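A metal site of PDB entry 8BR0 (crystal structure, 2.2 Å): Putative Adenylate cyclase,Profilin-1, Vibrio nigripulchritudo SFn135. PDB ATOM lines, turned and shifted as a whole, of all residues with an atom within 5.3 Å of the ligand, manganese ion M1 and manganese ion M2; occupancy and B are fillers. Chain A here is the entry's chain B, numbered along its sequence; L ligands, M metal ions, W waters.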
ATOM      1  N   ARG A  60     -28.211  16.961  15.876  1.00  0.00           N
ATOM      2  CA  ARG A  60     -27.062  17.747  15.457  1.00  0.00           C
ATOM      3  C   ARG A  60     -26.373  17.094  14.238  1.00  0.00           C
ATOM      4  O   ARG A  60     -26.666  15.943  13.904  1.00  0.00           O
ATOM      5  CB  ARG A  60     -26.096  17.912  16.641  1.00  0.00           C
ATOM      6  CG  ARG A  60     -26.591  18.858  17.739  1.00  0.00           C
ATOM      7  CD  ARG A  60     -25.587  18.922  18.886  1.00  0.00           C
ATOM      8  NE  ARG A  60     -24.274  19.357  18.372  1.00  0.00           N
ATOM      9  CZ  ARG A  60     -23.119  18.743  18.604  1.00  0.00           C
ATOM     10  NH1 ARG A  60     -23.058  17.708  19.432  1.00  0.00           N
ATOM     11  NH2 ARG A  60     -22.012  19.194  18.038  1.00  0.00           N
ATOM     12  N   LYS A  78     -19.665   6.891  20.458  1.00  0.00           N
ATOM     13  CA  LYS A  78     -19.186   7.617  21.626  1.00  0.00           C
ATOM     14  C   LYS A  78     -20.251   8.282  22.496  1.00  0.00           C
ATOM     15  O   LYS A  78     -21.094   9.054  22.016  1.00  0.00           O
ATOM     16  CB  LYS A  78     -18.152   8.664  21.175  1.00  0.00           C
ATOM     17  CG  LYS A  78     -18.632   9.544  20.024  1.00  0.00           C
ATOM     18  CD  LYS A  78     -17.713  10.734  19.712  1.00  0.00           C
ATOM     19  CE  LYS A  78     -17.867  11.812  20.742  1.00  0.00           C
ATOM     20  NZ  LYS A  78     -17.096  13.056  20.371  1.00  0.00           N
ATOM     21  N   LEU A  80     -20.921  10.181  26.633  1.00  0.00           N
ATOM     22  CA  LEU A  80     -20.326  11.248  27.422  1.00  0.00           C
ATOM     23  C   LEU A  80     -18.955  10.881  28.029  1.00  0.00           C
ATOM     24  O   LEU A  80     -18.226  11.777  28.415  1.00  0.00           O
ATOM     25  CB  LEU A  80     -21.289  11.777  28.510  1.00  0.00           C
ATOM     26  CG  LEU A  80     -22.010  13.170  28.282  1.00  0.00           C
ATOM     27  CD1 LEU A  80     -22.289  13.501  26.841  1.00  0.00           C
ATOM     28  CD2 LEU A  80     -23.291  13.302  29.129  1.00  0.00           C
ATOM     29  N   VAL A  82     -16.502   9.543  26.266  1.00  0.00           N
ATOM     30  CA  VAL A  82     -15.551   9.695  25.172  1.00  0.00           C
ATOM     31  C   VAL A  82     -15.781  11.091  24.610  1.00  0.00           C
ATOM     32  O   VAL A  82     -16.634  11.308  23.752  1.00  0.00           O
ATOM     33  CB  VAL A  82     -15.635   8.547  24.115  1.00  0.00           C
ATOM     34  CG1 VAL A  82     -14.795   8.847  22.864  1.00  0.00           C
ATOM     35  CG2 VAL A  82     -15.211   7.212  24.742  1.00  0.00           C
ATOM     36  N   LYS A  83     -15.092  12.085  25.203  1.00  0.00           N
ATOM     37  CA  LYS A  83     -15.261  13.475  24.768  1.00  0.00           C
ATOM     38  C   LYS A  83     -14.383  13.860  23.559  1.00  0.00           C
ATOM     39  O   LYS A  83     -14.653  14.856  22.898  1.00  0.00           O
ATOM     40  CB  LYS A  83     -15.105  14.448  25.913  1.00  0.00           C
ATOM     41  CG  LYS A  83     -16.169  14.327  26.990  1.00  0.00           C
ATOM     42  CD  LYS A  83     -15.859  15.377  28.079  1.00  0.00           C
ATOM     43  CE  LYS A  83     -16.500  15.097  29.403  1.00  0.00           C
ATOM     44  NZ  LYS A  83     -17.808  14.457  29.221  1.00  0.00           N
ATOM     45  N   ALA A  84     -13.382  13.033  23.218  1.00  0.00           N
ATOM     46  CA  ALA A  84     -12.523  13.191  22.060  1.00  0.00           C
ATOM     47  C   ALA A  84     -13.375  13.241  20.784  1.00  0.00           C
ATOM     48  O   ALA A  84     -14.347  12.494  20.673  1.00  0.00           O
ATOM     49  CB  ALA A  84     -11.582  11.999  21.978  1.00  0.00           C
ATOM     50  N   LYS A  85     -13.084  14.180  19.874  1.00  0.00           N
ATOM     51  CA  LYS A  85     -13.860  14.315  18.644  1.00  0.00           C
ATOM     52  C   LYS A  85     -13.579  13.266  17.609  1.00  0.00           C
ATOM     53  O   LYS A  85     -12.463  12.728  17.524  1.00  0.00           O
ATOM     54  CB  LYS A  85     -13.661  15.701  18.002  1.00  0.00           C
ATOM     55  CG  LYS A  85     -14.039  16.857  18.902  1.00  0.00           C
ATOM     56  CD  LYS A  85     -15.498  16.829  19.257  1.00  0.00           C
ATOM     57  CE  LYS A  85     -15.911  18.126  19.900  1.00  0.00           C
ATOM     58  NZ  LYS A  85     -17.253  17.972  20.490  1.00  0.00           N
ATOM     59  N   SER A  86     -14.562  13.037  16.745  1.00  0.00           N
ATOM     60  CA  SER A  86     -14.376  12.159  15.603  1.00  0.00           C
ATOM     61  C   SER A  86     -13.609  12.960  14.525  1.00  0.00           C
ATOM     62  O   SER A  86     -13.494  14.185  14.607  1.00  0.00           O
ATOM     63  CB  SER A  86     -15.741  11.701  15.084  1.00  0.00           C
ATOM     64  OG  SER A  86     -16.390  12.705  14.329  1.00  0.00           O
ATOM     65  N   LYS A 104     -11.643  16.376  13.730  1.00  0.00           N
ATOM     66  CA  LYS A 104     -12.268  17.505  13.078  1.00  0.00           C
ATOM     67  C   LYS A 104     -11.645  18.825  13.598  1.00  0.00           C
ATOM     68  O   LYS A 104     -10.933  18.826  14.613  1.00  0.00           O
ATOM     69  CB  LYS A 104     -13.784  17.448  13.292  1.00  0.00           C
ATOM     70  CG  LYS A 104     -14.176  17.696  14.737  1.00  0.00           C
ATOM     71  CD  LYS A 104     -15.658  17.739  14.918  1.00  0.00           C
ATOM     72  CE  LYS A 104     -16.238  16.370  14.773  1.00  0.00           C
ATOM     73  NZ  LYS A 104     -17.690  16.436  14.700  1.00  0.00           N
ATOM     74  N   ALA A 214     -19.072   8.384  15.520  1.00  0.00           N
ATOM     75  CA  ALA A 214     -19.783   9.494  16.126  1.00  0.00           C
ATOM     76  C   ALA A 214     -21.190   9.001  16.549  1.00  0.00           C
ATOM     77  O   ALA A 214     -21.708   7.993  16.038  1.00  0.00           O
ATOM     78  CB  ALA A 214     -19.928  10.596  15.103  1.00  0.00           C
ATOM     79  N   ASP A 215     -21.796   9.708  17.503  1.00  0.00           N
ATOM     80  CA  ASP A 215     -23.149   9.410  17.982  1.00  0.00           C
ATOM     81  C   ASP A 215     -24.170  10.312  17.265  1.00  0.00           C
ATOM     82  O   ASP A 215     -23.821  11.125  16.399  1.00  0.00           O
ATOM     83  CB  ASP A 215     -23.186   9.647  19.501  1.00  0.00           C
ATOM     84  CG  ASP A 215     -22.851  11.040  19.964  1.00  0.00           C
ATOM     85  OD1 ASP A 215     -21.980  11.688  19.349  1.00  0.00           O
ATOM     86  OD2 ASP A 215     -23.438  11.491  20.981  1.00  0.00           O
ATOM     87  N   ASP A 217     -26.389  13.215  18.295  1.00  0.00           N
ATOM     88  CA  ASP A 217     -26.612  14.116  19.403  1.00  0.00           C
ATOM     89  C   ASP A 217     -27.935  14.801  19.222  1.00  0.00           C
ATOM     90  O   ASP A 217     -28.066  15.581  18.285  1.00  0.00           O
ATOM     91  CB  ASP A 217     -25.533  15.170  19.460  1.00  0.00           C
ATOM     92  CG  ASP A 217     -24.201  14.634  19.858  1.00  0.00           C
ATOM     93  OD1 ASP A 217     -23.958  14.515  21.057  1.00  0.00           O
ATOM     94  OD2 ASP A 217     -23.388  14.349  18.979  1.00  0.00           O
ATOM     95  N   LEU A 274     -25.978  10.433  31.155  1.00  0.00           N
ATOM     96  CA  LEU A 274     -27.069  11.051  30.423  1.00  0.00           C
ATOM     97  C   LEU A 274     -26.966  12.555  30.395  1.00  0.00           C
ATOM     98  O   LEU A 274     -27.582  13.157  29.546  1.00  0.00           O
ATOM     99  CB  LEU A 274     -28.419  10.665  31.056  1.00  0.00           C
ATOM    100  CG  LEU A 274     -28.787   9.195  31.065  1.00  0.00           C
ATOM    101  CD1 LEU A 274     -30.058   8.978  31.857  1.00  0.00           C
ATOM    102  CD2 LEU A 274     -28.864   8.628  29.607  1.00  0.00           C
ATOM    103  N   GLY A 275     -26.275  13.170  31.354  1.00  0.00           N
ATOM    104  CA  GLY A 275     -26.197  14.610  31.461  1.00  0.00           C
ATOM    105  C   GLY A 275     -27.475  15.163  32.075  1.00  0.00           C
ATOM    106  O   GLY A 275     -28.092  14.527  32.943  1.00  0.00           O
ATOM    107  N   MET A 276     -27.891  16.332  31.641  1.00  0.00           N
ATOM    108  CA  MET A 276     -29.100  16.962  32.136  1.00  0.00           C
ATOM    109  C   MET A 276     -30.264  16.471  31.303  1.00  0.00           C
ATOM    110  O   MET A 276     -30.346  16.754  30.112  1.00  0.00           O
ATOM    111  CB  MET A 276     -28.970  18.472  32.033  1.00  0.00           C
ATOM    112  CG  MET A 276     -29.284  19.160  33.295  1.00  0.00           C
ATOM    113  SD  MET A 276     -27.889  19.120  34.384  1.00  0.00           S
ATOM    114  CE  MET A 276     -27.004  20.538  33.736  1.00  0.00           C
ATOM    115  N   HIS A 303     -27.199  10.353  25.459  1.00  0.00           N
ATOM    116  CA  HIS A 303     -27.386  11.346  26.513  1.00  0.00           C
ATOM    117  C   HIS A 303     -28.521  12.347  26.157  1.00  0.00           C
ATOM    118  O   HIS A 303     -29.134  12.241  25.106  1.00  0.00           O
ATOM    119  CB  HIS A 303     -26.021  12.082  26.744  1.00  0.00           C
ATOM    120  CG  HIS A 303     -25.365  12.600  25.497  1.00  0.00           C
ATOM    121  ND1 HIS A 303     -25.893  13.682  24.792  1.00  0.00           N
ATOM    122  CD2 HIS A 303     -24.279  12.130  24.831  1.00  0.00           C
ATOM    123  CE1 HIS A 303     -25.096  13.856  23.751  1.00  0.00           C
ATOM    124  NE2 HIS A 303     -24.107  12.951  23.719  1.00  0.00           N
ATOM    125  N   GLY A 304     -28.754  13.327  27.034  1.00  0.00           N
ATOM    126  CA  GLY A 304     -29.758  14.354  26.866  1.00  0.00           C
ATOM    127  C   GLY A 304     -29.492  15.300  25.713  1.00  0.00           C
ATOM    128  O   GLY A 304     -28.406  15.259  25.101  1.00  0.00           O
ATOM    129  N   ALA A 305     -30.472  16.182  25.447  1.00  0.00           N
ATOM    130  CA  ALA A 305     -30.395  17.122  24.353  1.00  0.00           C
ATOM    131  C   ALA A 305     -29.446  18.309  24.575  1.00  0.00           C
ATOM    132  O   ALA A 305     -29.120  18.672  25.724  1.00  0.00           O
ATOM    133  CB  ALA A 305     -31.790  17.612  23.960  1.00  0.00           C
ATOM    134  N   ASP A 306     -28.967  18.903  23.461  1.00  0.00           N
ATOM    135  CA  ASP A 306     -28.098  20.058  23.481  1.00  0.00           C
ATOM    136  C   ASP A 306     -28.759  21.262  24.155  1.00  0.00           C
ATOM    137  O   ASP A 306     -28.044  22.154  24.622  1.00  0.00           O
ATOM    138  CB  ASP A 306     -27.648  20.393  22.071  1.00  0.00           C
ATOM    139  CG  ASP A 306     -26.478  21.356  22.068  1.00  0.00           C
ATOM    140  OD1 ASP A 306     -25.393  20.970  22.548  1.00  0.00           O
ATOM    141  OD2 ASP A 306     -26.639  22.491  21.563  1.00  0.00           O
ATOM    142  N   ALA A 308     -30.051  21.364  27.001  1.00  0.00           N
ATOM    143  CA  ALA A 308     -29.687  21.371  28.413  1.00  0.00           C
ATOM    144  C   ALA A 308     -28.202  21.115  28.623  1.00  0.00           C
ATOM    145  O   ALA A 308     -27.814  20.772  29.718  1.00  0.00           O
ATOM    146  CB  ALA A 308     -30.461  20.301  29.138  1.00  0.00           C
ATOM    147  N   ASN A 309     -27.381  21.308  27.591  1.00  0.00           N
ATOM    148  CA  ASN A 309     -25.939  21.126  27.620  1.00  0.00           C
ATOM    149  C   ASN A 309     -25.290  22.476  27.916  1.00  0.00           C
ATOM    150  O   ASN A 309     -25.264  23.361  27.066  1.00  0.00           O
ATOM    151  CB  ASN A 309     -25.485  20.593  26.240  1.00  0.00           C
ATOM    152  CG  ASN A 309     -23.989  20.510  26.040  1.00  0.00           C
ATOM    153  OD1 ASN A 309     -23.187  20.628  26.968  1.00  0.00           O
ATOM    154  ND2 ASN A 309     -23.573  20.348  24.781  1.00  0.00           N
ATOM    155  N   PRO A 310     -24.691  22.626  29.126  1.00  0.00           N
ATOM    156  CA  PRO A 310     -24.022  23.893  29.445  1.00  0.00           C
ATOM    157  C   PRO A 310     -22.759  24.195  28.635  1.00  0.00           C
ATOM    158  O   PRO A 310     -22.250  25.315  28.693  1.00  0.00           O
ATOM    159  CB  PRO A 310     -23.721  23.766  30.941  1.00  0.00           C
ATOM    160  CG  PRO A 310     -23.660  22.330  31.194  1.00  0.00           C
ATOM    161  CD  PRO A 310     -24.626  21.681  30.250  1.00  0.00           C
ATOM    162  N   TYR A 311     -22.236  23.205  27.885  1.00  0.00           N
ATOM    163  CA  TYR A 311     -21.024  23.369  27.068  1.00  0.00           C
ATOM    164  C   TYR A 311     -21.353  23.405  25.565  1.00  0.00           C
ATOM    165  O   TYR A 311     -20.514  23.045  24.753  1.00  0.00           O
ATOM    166  CB  TYR A 311     -20.017  22.233  27.377  1.00  0.00           C
ATOM    167  CG  TYR A 311     -19.709  22.143  28.857  1.00  0.00           C
ATOM    168  CD1 TYR A 311     -18.936  23.121  29.479  1.00  0.00           C
ATOM    169  CD2 TYR A 311     -20.271  21.158  29.655  1.00  0.00           C
ATOM    170  CE1 TYR A 311     -18.693  23.086  30.844  1.00  0.00           C
ATOM    171  CE2 TYR A 311     -20.045  21.121  31.024  1.00  0.00           C
ATOM    172  CZ  TYR A 311     -19.243  22.090  31.613  1.00  0.00           C
ATOM    173  OH  TYR A 311     -19.003  22.069  32.979  1.00  0.00           O
ATOM    174  N   ASP A 316     -21.379  24.284  15.993  1.00  0.00           N
ATOM    175  CA  ASP A 316     -21.346  22.843  15.777  1.00  0.00           C
ATOM    176  C   ASP A 316     -22.716  22.154  15.803  1.00  0.00           C
ATOM    177  O   ASP A 316     -22.797  20.933  15.872  1.00  0.00           O
ATOM    178  CB  ASP A 316     -20.426  22.219  16.841  1.00  0.00           C
ATOM    179  CG  ASP A 316     -19.001  22.746  16.822  1.00  0.00           C
ATOM    180  OD1 ASP A 316     -18.606  23.367  15.797  1.00  0.00           O
ATOM    181  OD2 ASP A 316     -18.278  22.512  17.812  1.00  0.00           O
HETATM  182  N1  LIG L   1     -23.411  17.119  26.767  1.00  0.00           N
HETATM  183  C1  LIG L   1     -23.504  17.564  28.100  1.00  0.00           C
HETATM  184  N2  LIG L   1     -24.725  17.509  28.709  1.00  0.00           N
HETATM  185  C2  LIG L   1     -25.814  17.036  28.054  1.00  0.00           C
HETATM  186  C3  LIG L   1     -25.704  16.514  26.731  1.00  0.00           C
HETATM  187  C4  LIG L   1     -24.499  16.559  26.148  1.00  0.00           C
HETATM  188  O1  LIG L   1     -22.515  18.036  28.655  1.00  0.00           O
HETATM  189  N3  LIG L   1     -27.025  17.141  28.647  1.00  0.00           N
HETATM  190  C5  LIG L   1     -22.305  17.610  25.883  1.00  0.00           C
HETATM  191  C6  LIG L   1     -20.832  17.208  26.108  1.00  0.00           C
HETATM  192  O2  LIG L   1     -20.137  18.149  26.934  1.00  0.00           O
HETATM  193  C7  LIG L   1     -20.231  17.282  24.700  1.00  0.00           C
HETATM  194  C8  LIG L   1     -21.431  17.160  23.755  1.00  0.00           C
HETATM  195  O3  LIG L   1     -22.619  17.194  24.564  1.00  0.00           O
HETATM  196  C9  LIG L   1     -21.475  15.893  22.991  1.00  0.00           C
HETATM  197  O4  LIG L   1     -20.638  16.161  21.885  1.00  0.00           O
HETATM  198  P1  LIG L   1     -19.799  15.024  21.174  1.00  0.00           P
HETATM  199  O5  LIG L   1     -18.709  14.567  22.142  1.00  0.00           O
HETATM  200  O6  LIG L   1     -20.710  13.955  20.698  1.00  0.00           O
HETATM  201  O7  LIG L   1     -19.121  15.769  19.952  1.00  0.00           O
HETATM  202  P2  LIG L   1     -19.673  16.282  18.544  1.00  0.00           P
HETATM  203  O8  LIG L   1     -19.448  17.738  18.375  1.00  0.00           O
HETATM  204  O9  LIG L   1     -21.118  15.790  18.420  1.00  0.00           O
HETATM  205  O10 LIG L   1     -18.791  15.459  17.499  1.00  0.00           O
HETATM  206  P3  LIG L   1     -18.419  13.950  17.102  1.00  0.00           P
HETATM  207  O11 LIG L   1     -17.119  13.706  17.779  1.00  0.00           O
HETATM  208  O12 LIG L   1     -19.485  13.068  17.768  1.00  0.00           O
HETATM  209  O13 LIG L   1     -18.417  13.864  15.646  1.00  0.00           O
HETATM  210 MN    MN M   1     -22.596  13.301  22.044  1.00  0.00          MN
HETATM  211 MN    MN M   2     -21.511  13.668  18.541  1.00  0.00          MN
HETATM  212  O   HOH W   1     -22.504  16.566  16.164  1.00  0.00           O
HETATM  213  O   HOH W   2     -22.188  13.582  16.348  1.00  0.00           O
HETATM  214  O   HOH W   3     -24.601  18.066  21.918  1.00  0.00           O
HETATM  215  O   HOH W   4     -19.245  12.703  24.097  1.00  0.00           O
HETATM  216  O   HOH W   5     -16.810  16.228  22.798  1.00  0.00           O
HETATM  217  O   HOH W   6     -20.550  13.749  13.926  1.00  0.00           O
HETATM  218  O   HOH W   7     -21.458  11.617  23.062  1.00  0.00           O
HETATM  219  O   HOH W   8     -20.213  16.672  28.936  1.00  0.00           O
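The side-chain amide oxygen (OD1) of Asn 309 lies within hydrogen-bond range of the backbone NH (N) of Tyr 311 (2.9 Å). The side-chain carboxylate (OD1) of Asp 306 is in hydrogen-bond range of the side-chain amide nitrogen (ND2) of Asn 309 (2.9 Å). The side-chain amino group (NZ) of Lys 83 sits at hydrogen-bond distance from the backbone carbonyl oxygen (O) of Leu 80, at 2.8 Å. The guanidinium group (NH2) of Arg 60 lies within hydrogen-bond range of the backbone carbonyl oxygen (O) of Asp 316 (2.9 Å). The side-chain amino group (NZ) of Lys 78 sits at hydrogen-bond distance from the backbone carbonyl oxygen (O) of Ala 84, at 2.8 Å. The backbone carbonyl oxygen of Ser 86 is in hydrogen-bond range of the backbone NH of Lys 104 (3.0 Å). The backbone NH (N) of Gly 304 is in hydrogen-bond range of the backbone carbonyl oxygen (O) of Leu 274 (2.8 Å). O of Asp 217 is in hydrogen-bond range of N of Arg 60, at 2.8 Å.
A nitrogen (N3) of the ligand sits close to the backbone NH (N) of Met 276 (3.2 Å). Merely in contact with the ligand: Leu 80 (3.8 Å), Ala 214 (3.6 Å), Gly 275 (3.9 Å), Gly 304 (3.4 Å), Ala 305 (3.9 Å), Ala 308 (3.9 Å) and Tyr 311 (3.97 Å). 17 residues have an atom within 4 Å of the ligand: Arg 60, Lys 78, Leu 80, Lys 85, Ser 86, Lys 104, Ala 214, Asp 215, Asp 217, Gly 275, Met 276, His 303, Gly 304, Ala 305, Ala 308, Asn 309 and Tyr 311. The nearest printed residue that does not touch the ligand is Leu 274 (4.1 Å).
Manganese ion M1 is bound by OD1 of Asp 217, OD2 of Asp 215, water W7, NE2 of His 303 and O6 of the ligand.
Water W8 lies within hydrogen-bond range of an oxygen (O2) of the ligand (2.5 Å) and the side-chain amino group (NZ) of Lys 83 (3.3 Å). Water W5 lies within hydrogen-bond range of O of Lys 83 (2.6 Å), O5 of the ligand (2.6 Å) and NZ of Lys 85 (2.9 Å). Water W4 bridges O5 of the ligand and O of Val 82. Water W3 lies within hydrogen-bond range of the guanidinium group of Arg 60 (2.9 Å), the side-chain carboxylate of Asp 306 (3.1 Å) and an oxygen (O3) of the ligand (3.4 Å).
Within 4 Å of manganese ion M1: Asp 215, Asp 217 and His 303. The nearest printed residue that does not touch manganese ion M1 is Lys 78 (4.5 Å).
Manganese ion M2 is bound by OD2 of Asp 217 (2.0 Å), O9 of the ligand (2.2 Å), OD1 of Asp 215 (2.2 Å), O12 of the ligand (2.2 Å), water W2 (2.3 Å) and O6 of the ligand (2.3 Å).
NZ of Lys 78 lies within salt-bridge range of O11 of the ligand. The side-chain hydroxyl (OG) of Ser 86 lies within hydrogen-bond range of an oxygen (O13) of the ligand (2.7 Å). The backbone NH (N) of Ser 86 lies within hydrogen-bond range of an oxygen (O11) of the ligand (2.8 Å). An oxygen (O8) of the ligand lies within salt-bridge range of the guanidinium group of Arg 60, at 3.0 Å. The side-chain amino group (NZ) of Lys 104 is in salt-bridge range of an oxygen (O13) of the ligand, at 2.8 Å. The side-chain amide oxygen of Asn 309 lies close to an oxygen (O1) of the ligand, at 3.2 Å. The side-chain amino group (NZ) of Lys 85 lies within salt-bridge range of an oxygen (O8) of the ligand (3.1 Å).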
